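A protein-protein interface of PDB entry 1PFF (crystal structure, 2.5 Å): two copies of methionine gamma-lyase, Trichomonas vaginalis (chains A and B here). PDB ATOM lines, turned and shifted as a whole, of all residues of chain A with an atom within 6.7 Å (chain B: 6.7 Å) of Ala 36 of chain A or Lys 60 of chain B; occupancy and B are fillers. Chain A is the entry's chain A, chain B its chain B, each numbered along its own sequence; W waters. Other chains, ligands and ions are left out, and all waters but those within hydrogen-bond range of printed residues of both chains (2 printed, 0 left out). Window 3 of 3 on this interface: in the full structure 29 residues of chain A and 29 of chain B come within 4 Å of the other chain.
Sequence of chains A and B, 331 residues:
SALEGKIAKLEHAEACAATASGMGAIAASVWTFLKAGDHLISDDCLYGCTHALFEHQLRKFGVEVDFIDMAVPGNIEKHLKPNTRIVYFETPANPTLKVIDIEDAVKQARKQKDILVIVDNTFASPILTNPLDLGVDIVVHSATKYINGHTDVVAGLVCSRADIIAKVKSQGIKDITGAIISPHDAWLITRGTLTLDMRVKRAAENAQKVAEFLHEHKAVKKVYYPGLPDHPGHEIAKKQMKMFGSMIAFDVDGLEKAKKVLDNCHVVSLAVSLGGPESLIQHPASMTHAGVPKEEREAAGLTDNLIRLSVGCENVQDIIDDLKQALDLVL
O of Trp 31 of chain A lies within hydrogen-bond range of NZ of Lys 60 of chain B, at 2.7 Å. O of Thr 32 of chain A lies within hydrogen-bond range of NZ of Lys 60 of chain B, 3.1 Å away. The backbone carbonyl oxygen of Leu 34 of chain A is in hydrogen-bond range of the side-chain amino group of Lys 60 of chain B (3.0 Å). N of Ala 36 of chain A sits at hydrogen-bond distance from O of Lys 60 of chain B, at 3.0 Å. The side-chain amide oxygen (OE1) of Gln 171 of chain A is in hydrogen-bond range of the side-chain amide nitrogen (NE2) of Gln 57 of chain B, at 3.1 Å. NE1 of Trp 31 of chain B lies within hydrogen-bond range of O of Ile 176 of chain A, 2.9 Å away.
The side-chain amino group of Lys 35 of chain A lies within salt-bridge range of the side-chain carboxylate of Asp 38 of chain A (3.0 Å). O of Gln 171 of chain A is in hydrogen-bond range of N of Ile 176 of chain A (2.8 Å). OE1 of Gln 57 of chain B sits close to NZ of Lys 60 of chain B.
Trp 31 of chain A touches Phe 61 of chain B. Leu 34 of chain A touches Phe 61 of chain B. Lys 35 of chain A touches Lys 60 of chain B. CA of Lys 35 of chain A touches CE1 of Phe 61 of chain B, 3.7 Å away. N of Ala 36 of chain A touches CD1 of Phe 61 of chain B, at 3.8 Å. Trp 31 of chain B touches Phe 61 of chain A (CE3 to CZ, 3.5 Å). CD1 of Phe 61 of chain A touches N of Ala 36 of chain B, at 3.7 Å. CD1 of Phe 61 of chain A touches O of Phe 61 of chain B, 3.6 Å away. Gln 57 of chain B touches Ile 176 of chain A.
Of the printed residues of chain B, Ala 36 of chain A touches Lys 60 (3.0 Å) and Phe 61 (3.8 Å). Of the printed residues of chain B, Phe 61 of chain A touches Trp 31, Ala 36 and Phe 61. Printed residues of chain B within 4 Å of Ile 176 of chain A: Trp 31 and Gln 57. Printed residues of chain A within 4 Å of Gln 57 of chain B: Gln 171 (3.1 Å) and Ile 176 (3.4 Å). Lys 60 of chain B touches just these residues of chain A: Trp 31, Thr 32, Leu 34, Lys 35 and Ala 36.
Of the 12 printed residues of chain B, 5 touch a printed residue of chain A. Printed residues of chain B that touch a printed residue of chain A: Trp 31, Ala 36, Gln 57, Lys 60 and Phe 61. Hydrophobic or aromatic side chains of chain A within 4 Å of the printed part of chain B: Trp 31, Ala 36, Phe 61 and Ile 176. Among the printed residues, 15 pairs touch across the chains. Among the printed residues, no Asp or Glu carboxylate lies within 4 Å of a Lys or Arg side-chain nitrogen of the other chain.
Trp 31 of chain A touches Phe 61 of chain B, and with the chains exchanged Phe 61 of chain A touches Trp 31 of chain B. Ala 36 of chain A touches Phe 61 of chain B, and with the chains exchanged Phe 61 of chain A touches Ala 36 of chain B. Phe 61 of chain A touches its own counterpart, Phe 61 of chain B. Positions printed for both chains: 31, 36, 61, 62 and 63.
Water W2 lies within hydrogen-bond range of the side-chain amide oxygen of Gln 171 of chain A (2.5 Å), the side-chain amino group of Lys 60 of chain B (2.7 Å) and the side-chain amide oxygen of Gln 57 of chain B (3.2 Å). Water W1 lies within hydrogen-bond range of O of Lys 60 of chain B (3.0 Å) and O of Ala 36 of chain A (3.3 Å).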
ATOM      1  N   VAL A  30       8.569   7.463  14.318  1.00  0.00           N
ATOM      2  CA  VAL A  30       7.665   8.544  13.898  1.00  0.00           C
ATOM      3  C   VAL A  30       6.380   8.095  13.199  1.00  0.00           C
ATOM      4  O   VAL A  30       5.303   8.568  13.557  1.00  0.00           O
ATOM      5  CB  VAL A  30       8.374   9.695  13.101  1.00  0.00           C
ATOM      6  CG1 VAL A  30       9.538  10.273  13.907  1.00  0.00           C
ATOM      7  CG2 VAL A  30       8.815   9.250  11.705  1.00  0.00           C
ATOM      8  N   TRP A  31       6.467   7.188  12.223  1.00  0.00           N
ATOM      9  CA  TRP A  31       5.247   6.757  11.527  1.00  0.00           C
ATOM     10  C   TRP A  31       4.277   6.066  12.499  1.00  0.00           C
ATOM     11  O   TRP A  31       3.066   6.187  12.357  1.00  0.00           O
ATOM     12  CB  TRP A  31       5.543   5.800  10.369  1.00  0.00           C
ATOM     13  CG  TRP A  31       6.289   6.357   9.177  1.00  0.00           C
ATOM     14  CD1 TRP A  31       7.578   6.065   8.812  1.00  0.00           C
ATOM     15  CD2 TRP A  31       5.776   7.225   8.156  1.00  0.00           C
ATOM     16  NE1 TRP A  31       7.904   6.715   7.644  1.00  0.00           N
ATOM     17  CE2 TRP A  31       6.820   7.446   7.225  1.00  0.00           C
ATOM     18  CE3 TRP A  31       4.546   7.863   7.943  1.00  0.00           C
ATOM     19  CZ2 TRP A  31       6.667   8.263   6.096  1.00  0.00           C
ATOM     20  CZ3 TRP A  31       4.393   8.679   6.814  1.00  0.00           C
ATOM     21  CH2 TRP A  31       5.455   8.866   5.907  1.00  0.00           C
ATOM     22  N   THR A  32       4.814   5.338  13.482  1.00  0.00           N
ATOM     23  CA  THR A  32       3.981   4.621  14.453  1.00  0.00           C
ATOM     24  C   THR A  32       3.069   5.546  15.264  1.00  0.00           C
ATOM     25  O   THR A  32       1.928   5.186  15.592  1.00  0.00           O
ATOM     26  CB  THR A  32       4.883   3.809  15.409  1.00  0.00           C
ATOM     27  OG1 THR A  32       5.571   2.798  14.664  1.00  0.00           O
ATOM     28  CG2 THR A  32       4.054   3.014  16.420  1.00  0.00           C
ATOM     29  N   PHE A  33       3.582   6.729  15.591  1.00  0.00           N
ATOM     30  CA  PHE A  33       2.919   7.616  16.550  1.00  0.00           C
ATOM     31  C   PHE A  33       2.298   8.863  15.931  1.00  0.00           C
ATOM     32  O   PHE A  33       1.861   9.787  16.638  1.00  0.00           O
ATOM     33  CB  PHE A  33       3.862   7.943  17.720  1.00  0.00           C
ATOM     34  CG  PHE A  33       4.229   6.727  18.537  1.00  0.00           C
ATOM     35  CD1 PHE A  33       5.511   6.179  18.466  1.00  0.00           C
ATOM     36  CD2 PHE A  33       3.279   6.101  19.332  1.00  0.00           C
ATOM     37  CE1 PHE A  33       5.843   5.026  19.198  1.00  0.00           C
ATOM     38  CE2 PHE A  33       3.601   4.960  20.076  1.00  0.00           C
ATOM     39  CZ  PHE A  33       4.885   4.423  20.002  1.00  0.00           C
ATOM     40  N   LEU A  34       2.236   8.864  14.605  1.00  0.00           N
ATOM     41  CA  LEU A  34       1.606   9.943  13.853  1.00  0.00           C
ATOM     42  C   LEU A  34       0.436   9.405  13.038  1.00  0.00           C
ATOM     43  O   LEU A  34       0.311   8.197  12.838  1.00  0.00           O
ATOM     44  CB  LEU A  34       2.621  10.621  12.916  1.00  0.00           C
ATOM     45  CG  LEU A  34       3.727  11.454  13.578  1.00  0.00           C
ATOM     46  CD1 LEU A  34       4.753  11.927  12.547  1.00  0.00           C
ATOM     47  CD2 LEU A  34       3.180  12.649  14.415  1.00  0.00           C
ATOM     48  N   LYS A  35      -0.404  10.326  12.577  1.00  0.00           N
ATOM     49  CA  LYS A  35      -1.473  10.047  11.626  1.00  0.00           C
ATOM     50  C   LYS A  35      -1.758  11.335  10.871  1.00  0.00           C
ATOM     51  O   LYS A  35      -1.329  12.418  11.293  1.00  0.00           O
ATOM     52  CB  LYS A  35      -2.735   9.529  12.326  1.00  0.00           C
ATOM     53  CG  LYS A  35      -3.305  10.446  13.395  1.00  0.00           C
ATOM     54  CD  LYS A  35      -4.594   9.893  13.946  1.00  0.00           C
ATOM     55  CE  LYS A  35      -4.854  10.415  15.349  1.00  0.00           C
ATOM     56  NZ  LYS A  35      -4.681  11.890  15.485  1.00  0.00           N
ATOM     57  N   ALA A  36      -2.455  11.232   9.747  1.00  0.00           N
ATOM     58  CA  ALA A  36      -2.857  12.428   9.012  1.00  0.00           C
ATOM     59  C   ALA A  36      -3.613  13.333   9.982  1.00  0.00           C
ATOM     60  O   ALA A  36      -4.477  12.863  10.731  1.00  0.00           O
ATOM     61  CB  ALA A  36      -3.740  12.059   7.830  1.00  0.00           C
ATOM     62  N   GLY A  37      -3.275  14.618   9.977  1.00  0.00           N
ATOM     63  CA  GLY A  37      -3.871  15.573  10.894  1.00  0.00           C
ATOM     64  C   GLY A  37      -3.028  15.904  12.123  1.00  0.00           C
ATOM     65  O   GLY A  37      -3.373  16.834  12.872  1.00  0.00           O
ATOM     66  N   ASP A  38      -1.951  15.153  12.344  1.00  0.00           N
ATOM     67  CA  ASP A  38      -1.027  15.411  13.457  1.00  0.00           C
ATOM     68  C   ASP A  38       0.003  16.482  13.083  1.00  0.00           C
ATOM     69  O   ASP A  38       0.098  16.881  11.923  1.00  0.00           O
ATOM     70  CB  ASP A  38      -0.277  14.134  13.858  1.00  0.00           C
ATOM     71  CG  ASP A  38      -1.126  13.172  14.660  1.00  0.00           C
ATOM     72  OD1 ASP A  38      -2.249  13.533  15.091  1.00  0.00           O
ATOM     73  OD2 ASP A  38      -0.735  12.018  14.917  1.00  0.00           O
ATOM     74  N   PHE A  61       1.531  12.833   3.454  1.00  0.00           N
ATOM     75  CA  PHE A  61       0.518  12.043   4.164  1.00  0.00           C
ATOM     76  C   PHE A  61      -0.232  12.843   5.245  1.00  0.00           C
ATOM     77  O   PHE A  61      -0.707  12.275   6.232  1.00  0.00           O
ATOM     78  CB  PHE A  61       1.136  10.763   4.743  1.00  0.00           C
ATOM     79  CG  PHE A  61       1.486   9.748   3.696  1.00  0.00           C
ATOM     80  CD1 PHE A  61       0.486   9.138   2.936  1.00  0.00           C
ATOM     81  CD2 PHE A  61       2.810   9.439   3.430  1.00  0.00           C
ATOM     82  CE1 PHE A  61       0.813   8.218   1.934  1.00  0.00           C
ATOM     83  CE2 PHE A  61       3.142   8.501   2.445  1.00  0.00           C
ATOM     84  CZ  PHE A  61       2.142   7.902   1.691  1.00  0.00           C
ATOM     85  N   GLY A  62      -0.311  14.161   5.061  1.00  0.00           N
ATOM     86  CA  GLY A  62      -1.163  15.011   5.887  1.00  0.00           C
ATOM     87  C   GLY A  62      -0.672  15.381   7.280  1.00  0.00           C
ATOM     88  O   GLY A  62      -1.466  15.836   8.112  1.00  0.00           O
ATOM     89  N   VAL A  63       0.620  15.180   7.538  1.00  0.00           N
ATOM     90  CA  VAL A  63       1.248  15.604   8.792  1.00  0.00           C
ATOM     91  C   VAL A  63       1.795  17.017   8.590  1.00  0.00           C
ATOM     92  O   VAL A  63       2.480  17.285   7.606  1.00  0.00           O
ATOM     93  CB  VAL A  63       2.404  14.657   9.216  1.00  0.00           C
ATOM     94  CG1 VAL A  63       3.094  15.156  10.496  1.00  0.00           C
ATOM     95  CG2 VAL A  63       1.903  13.219   9.412  1.00  0.00           C
ATOM     96  N   GLN A 171       4.047  -2.544  15.124  1.00  0.00           N
ATOM     97  CA  GLN A 171       3.542  -1.672  14.063  1.00  0.00           C
ATOM     98  C   GLN A 171       4.670  -1.071  13.222  1.00  0.00           C
ATOM     99  O   GLN A 171       4.760  -1.329  12.029  1.00  0.00           O
ATOM    100  CB  GLN A 171       2.640  -0.582  14.644  1.00  0.00           C
ATOM    101  CG  GLN A 171       1.438  -1.136  15.399  1.00  0.00           C
ATOM    102  CD  GLN A 171       0.436  -0.069  15.739  1.00  0.00           C
ATOM    103  OE1 GLN A 171       0.171   0.813  14.922  1.00  0.00           O
ATOM    104  NE2 GLN A 171      -0.136  -0.140  16.943  1.00  0.00           N
ATOM    105  N   ILE A 176       4.796  -1.148   9.214  1.00  0.00           N
ATOM    106  CA  ILE A 176       5.007   0.108   8.495  1.00  0.00           C
ATOM    107  C   ILE A 176       6.264   0.129   7.623  1.00  0.00           C
ATOM    108  O   ILE A 176       6.189   0.439   6.430  1.00  0.00           O
ATOM    109  CB  ILE A 176       4.977   1.323   9.461  1.00  0.00           C
ATOM    110  CG1 ILE A 176       3.578   1.485  10.075  1.00  0.00           C
ATOM    111  CG2 ILE A 176       5.365   2.600   8.724  1.00  0.00           C
ATOM    112  CD1 ILE A 176       3.565   2.250  11.413  1.00  0.00           C
ATOM    113  N   TRP B  31       4.295   3.108  -0.010  1.00  0.00           N
ATOM    114  CA  TRP B  31       4.457   4.450   0.572  1.00  0.00           C
ATOM    115  C   TRP B  31       5.060   5.437  -0.445  1.00  0.00           C
ATOM    116  O   TRP B  31       4.775   6.640  -0.405  1.00  0.00           O
ATOM    117  CB  TRP B  31       5.343   4.432   1.820  1.00  0.00           C
ATOM    118  CG  TRP B  31       4.803   3.725   3.062  1.00  0.00           C
ATOM    119  CD1 TRP B  31       5.354   2.635   3.678  1.00  0.00           C
ATOM    120  CD2 TRP B  31       3.658   4.088   3.860  1.00  0.00           C
ATOM    121  NE1 TRP B  31       4.622   2.283   4.790  1.00  0.00           N
ATOM    122  CE2 TRP B  31       3.572   3.151   4.926  1.00  0.00           C
ATOM    123  CE3 TRP B  31       2.692   5.107   3.787  1.00  0.00           C
ATOM    124  CZ2 TRP B  31       2.566   3.200   5.900  1.00  0.00           C
ATOM    125  CZ3 TRP B  31       1.684   5.156   4.760  1.00  0.00           C
ATOM    126  CH2 TRP B  31       1.633   4.199   5.803  1.00  0.00           C
ATOM    127  N   ALA B  36      -1.751  11.194   0.810  1.00  0.00           N
ATOM    128  CA  ALA B  36      -3.085  11.385   1.379  1.00  0.00           C
ATOM    129  C   ALA B  36      -4.094  11.706   0.273  1.00  0.00           C
ATOM    130  O   ALA B  36      -3.823  12.525  -0.613  1.00  0.00           O
ATOM    131  CB  ALA B  36      -3.073  12.484   2.430  1.00  0.00           C
ATOM    132  N   PHE B  54      -2.179  -2.193   5.135  1.00  0.00           N
ATOM    133  CA  PHE B  54      -3.263  -1.571   4.369  1.00  0.00           C
ATOM    134  C   PHE B  54      -4.429  -1.103   5.240  1.00  0.00           C
ATOM    135  O   PHE B  54      -4.840   0.056   5.156  1.00  0.00           O
ATOM    136  CB  PHE B  54      -3.785  -2.534   3.294  1.00  0.00           C
ATOM    137  CG  PHE B  54      -2.769  -2.892   2.232  1.00  0.00           C
ATOM    138  CD1 PHE B  54      -1.551  -2.223   2.131  1.00  0.00           C
ATOM    139  CD2 PHE B  54      -3.049  -3.913   1.319  1.00  0.00           C
ATOM    140  CE1 PHE B  54      -0.619  -2.563   1.135  1.00  0.00           C
ATOM    141  CE2 PHE B  54      -2.135  -4.266   0.331  1.00  0.00           C
ATOM    142  CZ  PHE B  54      -0.917  -3.587   0.234  1.00  0.00           C
ATOM    143  N   GLU B  55      -4.944  -2.002   6.078  1.00  0.00           N
ATOM    144  CA  GLU B  55      -6.151  -1.737   6.877  1.00  0.00           C
ATOM    145  C   GLU B  55      -5.951  -0.652   7.927  1.00  0.00           C
ATOM    146  O   GLU B  55      -6.847   0.164   8.177  1.00  0.00           O
ATOM    147  CB  GLU B  55      -6.639  -3.017   7.559  1.00  0.00           C
ATOM    148  CG  GLU B  55      -7.978  -2.878   8.285  1.00  0.00           C
ATOM    149  CD  GLU B  55      -8.288  -4.040   9.219  1.00  0.00           C
ATOM    150  OE1 GLU B  55      -7.680  -5.120   9.071  1.00  0.00           O
ATOM    151  OE2 GLU B  55      -9.153  -3.874  10.112  1.00  0.00           O
ATOM    152  N   HIS B  56      -4.780  -0.645   8.555  1.00  0.00           N
ATOM    153  CA  HIS B  56      -4.557   0.273   9.662  1.00  0.00           C
ATOM    154  C   HIS B  56      -3.661   1.447   9.309  1.00  0.00           C
ATOM    155  O   HIS B  56      -4.042   2.598   9.509  1.00  0.00           O
ATOM    156  CB  HIS B  56      -4.038  -0.487  10.885  1.00  0.00           C
ATOM    157  CG  HIS B  56      -5.105  -1.278  11.577  1.00  0.00           C
ATOM    158  ND1 HIS B  56      -6.095  -0.686  12.331  1.00  0.00           N
ATOM    159  CD2 HIS B  56      -5.359  -2.608  11.598  1.00  0.00           C
ATOM    160  CE1 HIS B  56      -6.904  -1.620  12.803  1.00  0.00           C
ATOM    161  NE2 HIS B  56      -6.480  -2.794  12.371  1.00  0.00           N
ATOM    162  N   GLN B  57      -2.494   1.153   8.745  1.00  0.00           N
ATOM    163  CA  GLN B  57      -1.466   2.168   8.532  1.00  0.00           C
ATOM    164  C   GLN B  57      -1.752   3.099   7.351  1.00  0.00           C
ATOM    165  O   GLN B  57      -1.700   4.318   7.504  1.00  0.00           O
ATOM    166  CB  GLN B  57      -0.082   1.508   8.444  1.00  0.00           C
ATOM    167  CG  GLN B  57       0.128   0.439   9.526  1.00  0.00           C
ATOM    168  CD  GLN B  57       0.092   0.992  10.953  1.00  0.00           C
ATOM    169  OE1 GLN B  57       0.128   2.201  11.160  1.00  0.00           O
ATOM    170  NE2 GLN B  57       0.041   0.098  11.934  1.00  0.00           N
ATOM    171  N   LEU B  58      -2.077   2.542   6.185  1.00  0.00           N
ATOM    172  CA  LEU B  58      -2.399   3.396   5.040  1.00  0.00           C
ATOM    173  C   LEU B  58      -3.572   4.316   5.384  1.00  0.00           C
ATOM    174  O   LEU B  58      -3.521   5.524   5.147  1.00  0.00           O
ATOM    175  CB  LEU B  58      -2.702   2.564   3.787  1.00  0.00           C
ATOM    176  CG  LEU B  58      -1.526   1.801   3.159  1.00  0.00           C
ATOM    177  CD1 LEU B  58      -1.947   1.217   1.807  1.00  0.00           C
ATOM    178  CD2 LEU B  58      -0.289   2.674   2.999  1.00  0.00           C
ATOM    179  N   ARG B  59      -4.608   3.737   5.981  1.00  0.00           N
ATOM    180  CA  ARG B  59      -5.811   4.483   6.342  1.00  0.00           C
ATOM    181  C   ARG B  59      -5.539   5.584   7.363  1.00  0.00           C
ATOM    182  O   ARG B  59      -6.149   6.650   7.307  1.00  0.00           O
ATOM    183  CB  ARG B  59      -6.892   3.540   6.871  1.00  0.00           C
ATOM    184  CG  ARG B  59      -7.586   2.722   5.782  1.00  0.00           C
ATOM    185  CD  ARG B  59      -8.716   1.856   6.331  1.00  0.00           C
ATOM    186  NE  ARG B  59      -9.524   1.261   5.269  1.00  0.00           N
ATOM    187  CZ  ARG B  59     -10.244   0.149   5.406  1.00  0.00           C
ATOM    188  NH1 ARG B  59     -10.251  -0.512   6.559  1.00  0.00           N
ATOM    189  NH2 ARG B  59     -10.955  -0.307   4.382  1.00  0.00           N
ATOM    190  N   LYS B  60      -4.607   5.319   8.276  1.00  0.00           N
ATOM    191  CA  LYS B  60      -4.189   6.280   9.291  1.00  0.00           C
ATOM    192  C   LYS B  60      -3.652   7.557   8.628  1.00  0.00           C
ATOM    193  O   LYS B  60      -3.793   8.658   9.176  1.00  0.00           O
ATOM    194  CB  LYS B  60      -3.103   5.612  10.141  1.00  0.00           C
ATOM    195  CG  LYS B  60      -2.552   6.391  11.257  1.00  0.00           C
ATOM    196  CD  LYS B  60      -1.772   5.494  12.190  1.00  0.00           C
ATOM    197  CE  LYS B  60      -0.356   5.319  11.703  1.00  0.00           C
ATOM    198  NZ  LYS B  60       0.558   5.191  12.862  1.00  0.00           N
ATOM    199  N   PHE B  61      -3.051   7.398   7.446  1.00  0.00           N
ATOM    200  CA  PHE B  61      -2.429   8.513   6.730  1.00  0.00           C
ATOM    201  C   PHE B  61      -3.243   9.002   5.532  1.00  0.00           C
ATOM    202  O   PHE B  61      -2.684   9.533   4.573  1.00  0.00           O
ATOM    203  CB  PHE B  61      -0.985   8.153   6.345  1.00  0.00           C
ATOM    204  CG  PHE B  61      -0.051   8.102   7.529  1.00  0.00           C
ATOM    205  CD1 PHE B  61       0.361   9.280   8.157  1.00  0.00           C
ATOM    206  CD2 PHE B  61       0.374   6.885   8.046  1.00  0.00           C
ATOM    207  CE1 PHE B  61       1.206   9.244   9.258  1.00  0.00           C
ATOM    208  CE2 PHE B  61       1.216   6.837   9.153  1.00  0.00           C
ATOM    209  CZ  PHE B  61       1.635   8.022   9.762  1.00  0.00           C
ATOM    210  N   GLY B  62      -4.564   8.818   5.606  1.00  0.00           N
ATOM    211  CA  GLY B  62      -5.496   9.406   4.657  1.00  0.00           C
ATOM    212  C   GLY B  62      -5.643   8.691   3.323  1.00  0.00           C
ATOM    213  O   GLY B  62      -6.163   9.271   2.358  1.00  0.00           O
ATOM    214  N   VAL B  63      -5.180   7.444   3.261  1.00  0.00           N
ATOM    215  CA  VAL B  63      -5.334   6.621   2.067  1.00  0.00           C
ATOM    216  C   VAL B  63      -6.618   5.792   2.177  1.00  0.00           C
ATOM    217  O   VAL B  63      -6.855   5.136   3.195  1.00  0.00           O
ATOM    218  CB  VAL B  63      -4.083   5.732   1.818  1.00  0.00           C
ATOM    219  CG1 VAL B  63      -4.277   4.818   0.604  1.00  0.00           C
ATOM    220  CG2 VAL B  63      -2.847   6.609   1.622  1.00  0.00           C
HETATM  221  O   HOH W   1      -6.211  10.066  10.257  1.00  0.00           O
HETATM  222  O   HOH W   2      -0.558   3.046  14.149  1.00  0.00           O
